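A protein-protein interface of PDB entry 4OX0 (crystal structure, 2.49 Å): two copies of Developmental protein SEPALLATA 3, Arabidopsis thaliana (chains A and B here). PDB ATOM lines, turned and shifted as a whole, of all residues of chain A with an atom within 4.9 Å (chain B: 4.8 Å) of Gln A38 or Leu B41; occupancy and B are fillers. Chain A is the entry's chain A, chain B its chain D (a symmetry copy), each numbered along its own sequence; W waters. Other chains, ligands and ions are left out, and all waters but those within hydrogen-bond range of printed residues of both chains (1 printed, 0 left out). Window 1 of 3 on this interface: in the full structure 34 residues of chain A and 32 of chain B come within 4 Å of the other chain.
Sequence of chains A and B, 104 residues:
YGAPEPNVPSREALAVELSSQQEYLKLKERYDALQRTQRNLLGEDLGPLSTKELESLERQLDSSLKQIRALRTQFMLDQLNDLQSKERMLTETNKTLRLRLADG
The side-chain hydroxyl (OG) of Ser A64 lies within hydrogen-bond range of the backbone NH (N) of Leu B42 (2.8 Å).
OE1 of Gln B38 sits close to O of Leu A34, 3.3 Å away.
OG of Ser A64 is in hydrogen-bond range of N of Gly B43, 3.3 Å away.
The side-chain hydroxyl of Thr A37 is in hydrogen-bond range of the side-chain amide oxygen of Gln B38 (3.5 Å).
The side-chain amide oxygen of Gln A38 lies close to the side-chain amide oxygen of Gln B38.
OG1 of Thr A37 lies within hydrogen-bond range of O of Leu A34, 2.8 Å away.
Leu A34 touches Leu B34 (CD2 to CD2, 3.7 Å).
CD1 of Leu B34 touches OE1 of Gln A35, at 3.4 Å.
NE2 of Gln A38 touches CG2 of Thr B37 (3.2 Å).
Leu B41 touches Gln A38.
Gln B38 touches Leu A41.
Gln B60 touches Leu A42 (CG to CD2, 3.1 Å).
Leu B41 touches Ser A64.
CD1 of Leu B61 touches OG of Ser A64, 3.5 Å away.
Printed residues of chain B within 4 Å of Leu A34: Leu B34 (3.7 Å) and Gln B38 (3.3 Å).
Gln A38 touches just these residues of chain B: Thr B37, Gln B38 and Leu B41.
Arg A39 touches none of the printed residues of chain B.
Printed residues of chain B within 4 Å of Ser A64: Leu B41, Leu B42, Gly B43 and Leu B61.
Printed residues of chain A within 4 Å of Gln B38: Leu A34 (3.3 Å), Thr A37 (3.5 Å), Gln A38 (3.1 Å) and Leu A41 (3.99 Å).
Printed residues of chain A within 4 Å of Leu B41: Gln A38 and Ser A64.
The nearest residue of chain B that does not touch Gln A38 is Leu B34 (4.2 Å).
The nearest printed residue of chain A that does not touch Gly B43 is Leu A41 (8.3 Å).
Of the 10 printed residues of chain A, 7 touch a printed residue of chain B.
Hydrophobic or aromatic side chains of chain A that line the printed part of chain B: Leu A34, Leu A41 and Leu A42.
Hydrophobic or aromatic side chains of chain B within 4 Å of the printed part of chain A: Leu B34, Leu B41 and Leu B61.
Among the printed residues, 13 pairs touch across the chains.
Leu B34 touches its own counterpart, Leu A34.
Thr A37 touches Gln B38, and with the chains exchanged Gln A38 touches Thr B37.
Gln A38 touches its own counterpart, Gln B38.
Gln A38 touches Leu B41, and with the chains exchanged Leu A41 touches Gln B38.
Water W1 lies within hydrogen-bond range of the backbone carbonyl oxygen of Leu A42 and the side-chain amide oxygen of Gln B60.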
ATOM      1  N   LEU A  34      15.545  -7.517 -13.591  1.00  0.00           N
ATOM      2  CA  LEU A  34      16.832  -7.886 -14.177  1.00  0.00           C
ATOM      3  C   LEU A  34      17.117  -9.352 -13.898  1.00  0.00           C
ATOM      4  O   LEU A  34      17.617 -10.051 -14.781  1.00  0.00           O
ATOM      5  CB  LEU A  34      17.955  -6.997 -13.597  1.00  0.00           C
ATOM      6  CG  LEU A  34      19.268  -6.937 -14.371  1.00  0.00           C
ATOM      7  CD1 LEU A  34      19.087  -6.207 -15.680  1.00  0.00           C
ATOM      8  CD2 LEU A  34      20.341  -6.236 -13.579  1.00  0.00           C
ATOM      9  N   GLN A  35      16.799  -9.808 -12.668  1.00  0.00           N
ATOM     10  CA  GLN A  35      16.971 -11.195 -12.238  1.00  0.00           C
ATOM     11  C   GLN A  35      15.999 -12.105 -13.004  1.00  0.00           C
ATOM     12  O   GLN A  35      16.369 -13.231 -13.319  1.00  0.00           O
ATOM     13  CB  GLN A  35      16.832 -11.323 -10.709  1.00  0.00           C
ATOM     14  CG  GLN A  35      17.062 -12.728 -10.126  1.00  0.00           C
ATOM     15  CD  GLN A  35      18.379 -13.377 -10.489  1.00  0.00           C
ATOM     16  OE1 GLN A  35      19.443 -12.761 -10.511  1.00  0.00           O
ATOM     17  NE2 GLN A  35      18.346 -14.662 -10.730  1.00  0.00           N
ATOM     18  N   ARG A  36      14.798 -11.598 -13.373  1.00  0.00           N
ATOM     19  CA  ARG A  36      13.820 -12.334 -14.176  1.00  0.00           C
ATOM     20  C   ARG A  36      14.368 -12.618 -15.580  1.00  0.00           C
ATOM     21  O   ARG A  36      14.398 -13.789 -16.006  1.00  0.00           O
ATOM     22  CB  ARG A  36      12.484 -11.587 -14.250  1.00  0.00           C
ATOM     23  CG  ARG A  36      11.561 -11.954 -13.104  1.00  0.00           C
ATOM     24  CD  ARG A  36      10.121 -11.556 -13.376  1.00  0.00           C
ATOM     25  NE  ARG A  36       9.948 -10.113 -13.562  1.00  0.00           N
ATOM     26  CZ  ARG A  36       9.841  -9.225 -12.575  1.00  0.00           C
ATOM     27  NH1 ARG A  36       9.907  -9.617 -11.303  1.00  0.00           N
ATOM     28  NH2 ARG A  36       9.677  -7.940 -12.848  1.00  0.00           N
ATOM     29  N   THR A  37      14.855 -11.548 -16.266  1.00  0.00           N
ATOM     30  CA  THR A  37      15.484 -11.615 -17.592  1.00  0.00           C
ATOM     31  C   THR A  37      16.718 -12.516 -17.552  1.00  0.00           C
ATOM     32  O   THR A  37      16.964 -13.274 -18.480  1.00  0.00           O
ATOM     33  CB  THR A  37      15.766 -10.199 -18.147  1.00  0.00           C
ATOM     34  OG1 THR A  37      16.255  -9.331 -17.128  1.00  0.00           O
ATOM     35  CG2 THR A  37      14.534  -9.561 -18.810  1.00  0.00           C
ATOM     36  N   GLN A  38      17.438 -12.485 -16.437  1.00  0.00           N
ATOM     37  CA  GLN A  38      18.630 -13.297 -16.225  1.00  0.00           C
ATOM     38  C   GLN A  38      18.294 -14.763 -16.024  1.00  0.00           C
ATOM     39  O   GLN A  38      19.151 -15.582 -16.271  1.00  0.00           O
ATOM     40  CB  GLN A  38      19.430 -12.775 -15.021  1.00  0.00           C
ATOM     41  CG  GLN A  38      20.752 -13.472 -14.831  1.00  0.00           C
ATOM     42  CD  GLN A  38      21.872 -12.930 -15.673  1.00  0.00           C
ATOM     43  OE1 GLN A  38      21.680 -12.124 -16.591  1.00  0.00           O
ATOM     44  NE2 GLN A  38      23.064 -13.439 -15.417  1.00  0.00           N
ATOM     45  N   ARG A  39      17.114 -15.097 -15.487  1.00  0.00           N
ATOM     46  CA  ARG A  39      16.751 -16.507 -15.283  1.00  0.00           C
ATOM     47  C   ARG A  39      16.406 -17.159 -16.616  1.00  0.00           C
ATOM     48  O   ARG A  39      16.760 -18.317 -16.841  1.00  0.00           O
ATOM     49  CB  ARG A  39      15.637 -16.671 -14.241  1.00  0.00           C
ATOM     50  CG  ARG A  39      16.102 -16.422 -12.779  1.00  0.00           C
ATOM     51  CD  ARG A  39      16.779 -17.622 -12.110  1.00  0.00           C
ATOM     52  NE  ARG A  39      15.855 -18.736 -11.870  1.00  0.00           N
ATOM     53  CZ  ARG A  39      16.229 -19.972 -11.549  1.00  0.00           C
ATOM     54  NH1 ARG A  39      17.517 -20.284 -11.464  1.00  0.00           N
ATOM     55  NH2 ARG A  39      15.318 -20.916 -11.359  1.00  0.00           N
ATOM     56  N   ASN A  40      15.790 -16.381 -17.526  1.00  0.00           N
ATOM     57  CA  ASN A  40      15.449 -16.775 -18.891  1.00  0.00           C
ATOM     58  C   ASN A  40      16.709 -17.130 -19.693  1.00  0.00           C
ATOM     59  O   ASN A  40      16.771 -18.219 -20.253  1.00  0.00           O
ATOM     60  CB  ASN A  40      14.600 -15.702 -19.553  1.00  0.00           C
ATOM     61  CG  ASN A  40      13.241 -15.589 -18.926  1.00  0.00           C
ATOM     62  OD1 ASN A  40      12.781 -16.494 -18.212  1.00  0.00           O
ATOM     63  ND2 ASN A  40      12.556 -14.495 -19.214  1.00  0.00           N
ATOM     64  N   LEU A  41      17.743 -16.250 -19.694  1.00  0.00           N
ATOM     65  CA  LEU A  41      19.090 -16.550 -20.247  1.00  0.00           C
ATOM     66  C   LEU A  41      19.573 -17.385 -19.085  1.00  0.00           C
ATOM     67  O   LEU A  41      19.317 -16.977 -17.973  1.00  0.00           O
ATOM     68  CB  LEU A  41      19.959 -15.281 -20.330  1.00  0.00           C
ATOM     69  CG  LEU A  41      19.264 -13.963 -20.601  1.00  0.00           C
ATOM     70  CD1 LEU A  41      20.095 -12.795 -20.102  1.00  0.00           C
ATOM     71  CD2 LEU A  41      18.905 -13.825 -22.055  1.00  0.00           C
ATOM     72  N   LEU A  42      20.162 -18.547 -19.276  1.00  0.00           N
ATOM     73  CA  LEU A  42      20.462 -19.521 -18.185  1.00  0.00           C
ATOM     74  C   LEU A  42      19.439 -20.665 -18.248  1.00  0.00           C
ATOM     75  O   LEU A  42      19.677 -21.709 -17.632  1.00  0.00           O
ATOM     76  CB  LEU A  42      20.541 -18.998 -16.714  1.00  0.00           C
ATOM     77  CG  LEU A  42      21.600 -17.960 -16.290  1.00  0.00           C
ATOM     78  CD1 LEU A  42      21.468 -17.648 -14.834  1.00  0.00           C
ATOM     79  CD2 LEU A  42      23.006 -18.355 -16.626  1.00  0.00           C
ATOM     80  N   SER A  64      24.677 -14.892 -29.634  1.00  0.00           N
ATOM     81  CA  SER A  64      25.513 -14.563 -28.498  1.00  0.00           C
ATOM     82  C   SER A  64      26.577 -15.654 -28.332  1.00  0.00           C
ATOM     83  O   SER A  64      27.739 -15.323 -28.214  1.00  0.00           O
ATOM     84  CB  SER A  64      24.618 -14.424 -27.264  1.00  0.00           C
ATOM     85  OG  SER A  64      25.296 -14.317 -26.029  1.00  0.00           O
ATOM     86  N   LEU B  34      25.142  -7.789 -11.680  1.00  0.00           N
ATOM     87  CA  LEU B  34      24.154  -8.600 -12.396  1.00  0.00           C
ATOM     88  C   LEU B  34      23.999  -8.056 -13.800  1.00  0.00           C
ATOM     89  O   LEU B  34      23.858  -8.836 -14.727  1.00  0.00           O
ATOM     90  CB  LEU B  34      22.792  -8.574 -11.671  1.00  0.00           C
ATOM     91  CG  LEU B  34      21.751  -9.631 -12.094  1.00  0.00           C
ATOM     92  CD1 LEU B  34      22.174 -11.015 -11.672  1.00  0.00           C
ATOM     93  CD2 LEU B  34      20.398  -9.327 -11.491  1.00  0.00           C
ATOM     94  N   THR B  37      27.062  -9.316 -15.876  1.00  0.00           N
ATOM     95  CA  THR B  37      26.856 -10.719 -16.242  1.00  0.00           C
ATOM     96  C   THR B  37      25.796 -10.823 -17.338  1.00  0.00           C
ATOM     97  O   THR B  37      25.948 -11.630 -18.261  1.00  0.00           O
ATOM     98  CB  THR B  37      26.504 -11.553 -14.991  1.00  0.00           C
ATOM     99  OG1 THR B  37      27.602 -11.491 -14.095  1.00  0.00           O
ATOM    100  CG2 THR B  37      26.212 -13.009 -15.308  1.00  0.00           C
ATOM    101  N   GLN B  38      24.748  -9.979 -17.253  1.00  0.00           N
ATOM    102  CA  GLN B  38      23.673  -9.936 -18.229  1.00  0.00           C
ATOM    103  C   GLN B  38      24.143  -9.429 -19.591  1.00  0.00           C
ATOM    104  O   GLN B  38      23.590  -9.842 -20.609  1.00  0.00           O
ATOM    105  CB  GLN B  38      22.523  -9.070 -17.727  1.00  0.00           C
ATOM    106  CG  GLN B  38      21.409  -9.051 -18.745  1.00  0.00           C
ATOM    107  CD  GLN B  38      20.069  -9.018 -18.160  1.00  0.00           C
ATOM    108  OE1 GLN B  38      19.699  -9.896 -17.383  1.00  0.00           O
ATOM    109  NE2 GLN B  38      19.288  -8.040 -18.581  1.00  0.00           N
ATOM    110  N   ARG B  39      25.094  -8.482 -19.612  1.00  0.00           N
ATOM    111  CA  ARG B  39      25.592  -7.937 -20.874  1.00  0.00           C
ATOM    112  C   ARG B  39      26.466  -8.961 -21.598  1.00  0.00           C
ATOM    113  O   ARG B  39      26.402  -9.050 -22.820  1.00  0.00           O
ATOM    114  CB  ARG B  39      26.332  -6.609 -20.647  1.00  0.00           C
ATOM    115  CG  ARG B  39      25.409  -5.427 -20.292  1.00  0.00           C
ATOM    116  CD  ARG B  39      24.763  -4.740 -21.489  1.00  0.00           C
ATOM    117  NE  ARG B  39      25.747  -4.025 -22.309  1.00  0.00           N
ATOM    118  CZ  ARG B  39      25.524  -3.579 -23.541  1.00  0.00           C
ATOM    119  NH1 ARG B  39      24.351  -3.789 -24.128  1.00  0.00           N
ATOM    120  NH2 ARG B  39      26.482  -2.956 -24.210  1.00  0.00           N
ATOM    121  N   ASN B  40      27.240  -9.752 -20.819  1.00  0.00           N
ATOM    122  CA  ASN B  40      28.138 -10.831 -21.246  1.00  0.00           C
ATOM    123  C   ASN B  40      27.375 -11.909 -22.029  1.00  0.00           C
ATOM    124  O   ASN B  40      27.683 -12.125 -23.200  1.00  0.00           O
ATOM    125  CB  ASN B  40      28.903 -11.371 -20.041  1.00  0.00           C
ATOM    126  CG  ASN B  40      29.919 -10.400 -19.520  1.00  0.00           C
ATOM    127  OD1 ASN B  40      30.245  -9.378 -20.158  1.00  0.00           O
ATOM    128  ND2 ASN B  40      30.507 -10.746 -18.387  1.00  0.00           N
ATOM    129  N   LEU B  41      26.326 -12.515 -21.411  1.00  0.00           N
ATOM    130  CA  LEU B  41      25.325 -13.378 -22.065  1.00  0.00           C
ATOM    131  C   LEU B  41      24.664 -12.266 -22.883  1.00  0.00           C
ATOM    132  O   LEU B  41      24.591 -11.171 -22.350  1.00  0.00           O
ATOM    133  CB  LEU B  41      24.314 -13.867 -21.015  1.00  0.00           C
ATOM    134  CG  LEU B  41      24.856 -14.530 -19.752  1.00  0.00           C
ATOM    135  CD1 LEU B  41      23.760 -14.688 -18.735  1.00  0.00           C
ATOM    136  CD2 LEU B  41      25.444 -15.916 -20.059  1.00  0.00           C
ATOM    137  N   LEU B  42      24.291 -12.443 -24.150  1.00  0.00           N
ATOM    138  CA  LEU B  42      23.793 -11.325 -25.012  1.00  0.00           C
ATOM    139  C   LEU B  42      24.934 -10.776 -25.871  1.00  0.00           C
ATOM    140  O   LEU B  42      24.677 -10.043 -26.831  1.00  0.00           O
ATOM    141  CB  LEU B  42      23.066 -10.143 -24.302  1.00  0.00           C
ATOM    142  CG  LEU B  42      21.734 -10.397 -23.540  1.00  0.00           C
ATOM    143  CD1 LEU B  42      21.227  -9.119 -22.891  1.00  0.00           C
ATOM    144  CD2 LEU B  42      20.652 -10.997 -24.456  1.00  0.00           C
ATOM    145  N   GLY B  43      26.169 -11.163 -25.526  1.00  0.00           N
ATOM    146  CA  GLY B  43      27.393 -10.880 -26.267  1.00  0.00           C
ATOM    147  C   GLY B  43      27.920  -9.460 -26.298  1.00  0.00           C
ATOM    148  O   GLY B  43      28.595  -9.081 -27.260  1.00  0.00           O
ATOM    149  N   LEU B  57      30.939 -18.792 -20.090  1.00  0.00           N
ATOM    150  CA  LEU B  57      29.777 -18.166 -20.732  1.00  0.00           C
ATOM    151  C   LEU B  57      29.227 -19.120 -21.814  1.00  0.00           C
ATOM    152  O   LEU B  57      28.016 -19.339 -21.895  1.00  0.00           O
ATOM    153  CB  LEU B  57      30.202 -16.841 -21.401  1.00  0.00           C
ATOM    154  CG  LEU B  57      29.705 -15.500 -20.835  1.00  0.00           C
ATOM    155  CD1 LEU B  57      30.336 -15.196 -19.494  1.00  0.00           C
ATOM    156  CD2 LEU B  57      30.073 -14.352 -21.764  1.00  0.00           C
ATOM    157  N   GLN B  60      27.454 -22.119 -20.308  1.00  0.00           N
ATOM    158  CA  GLN B  60      26.167 -21.720 -19.774  1.00  0.00           C
ATOM    159  C   GLN B  60      25.145 -21.467 -20.885  1.00  0.00           C
ATOM    160  O   GLN B  60      24.026 -21.949 -20.781  1.00  0.00           O
ATOM    161  CB  GLN B  60      26.319 -20.519 -18.841  1.00  0.00           C
ATOM    162  CG  GLN B  60      25.067 -20.160 -18.063  1.00  0.00           C
ATOM    163  CD  GLN B  60      24.280 -21.327 -17.507  1.00  0.00           C
ATOM    164  OE1 GLN B  60      23.208 -21.677 -18.021  1.00  0.00           O
ATOM    165  NE2 GLN B  60      24.738 -21.883 -16.393  1.00  0.00           N
ATOM    166  N   LEU B  61      25.540 -20.771 -21.968  1.00  0.00           N
ATOM    167  CA  LEU B  61      24.678 -20.508 -23.115  1.00  0.00           C
ATOM    168  C   LEU B  61      24.293 -21.780 -23.830  1.00  0.00           C
ATOM    169  O   LEU B  61      23.163 -21.888 -24.294  1.00  0.00           O
ATOM    170  CB  LEU B  61      25.348 -19.544 -24.096  1.00  0.00           C
ATOM    171  CG  LEU B  61      25.499 -18.133 -23.633  1.00  0.00           C
ATOM    172  CD1 LEU B  61      26.354 -17.321 -24.579  1.00  0.00           C
ATOM    173  CD2 LEU B  61      24.129 -17.478 -23.431  1.00  0.00           C
HETATM  174  O   HOH W   1      21.095 -23.839 -16.673  1.00  0.00           O
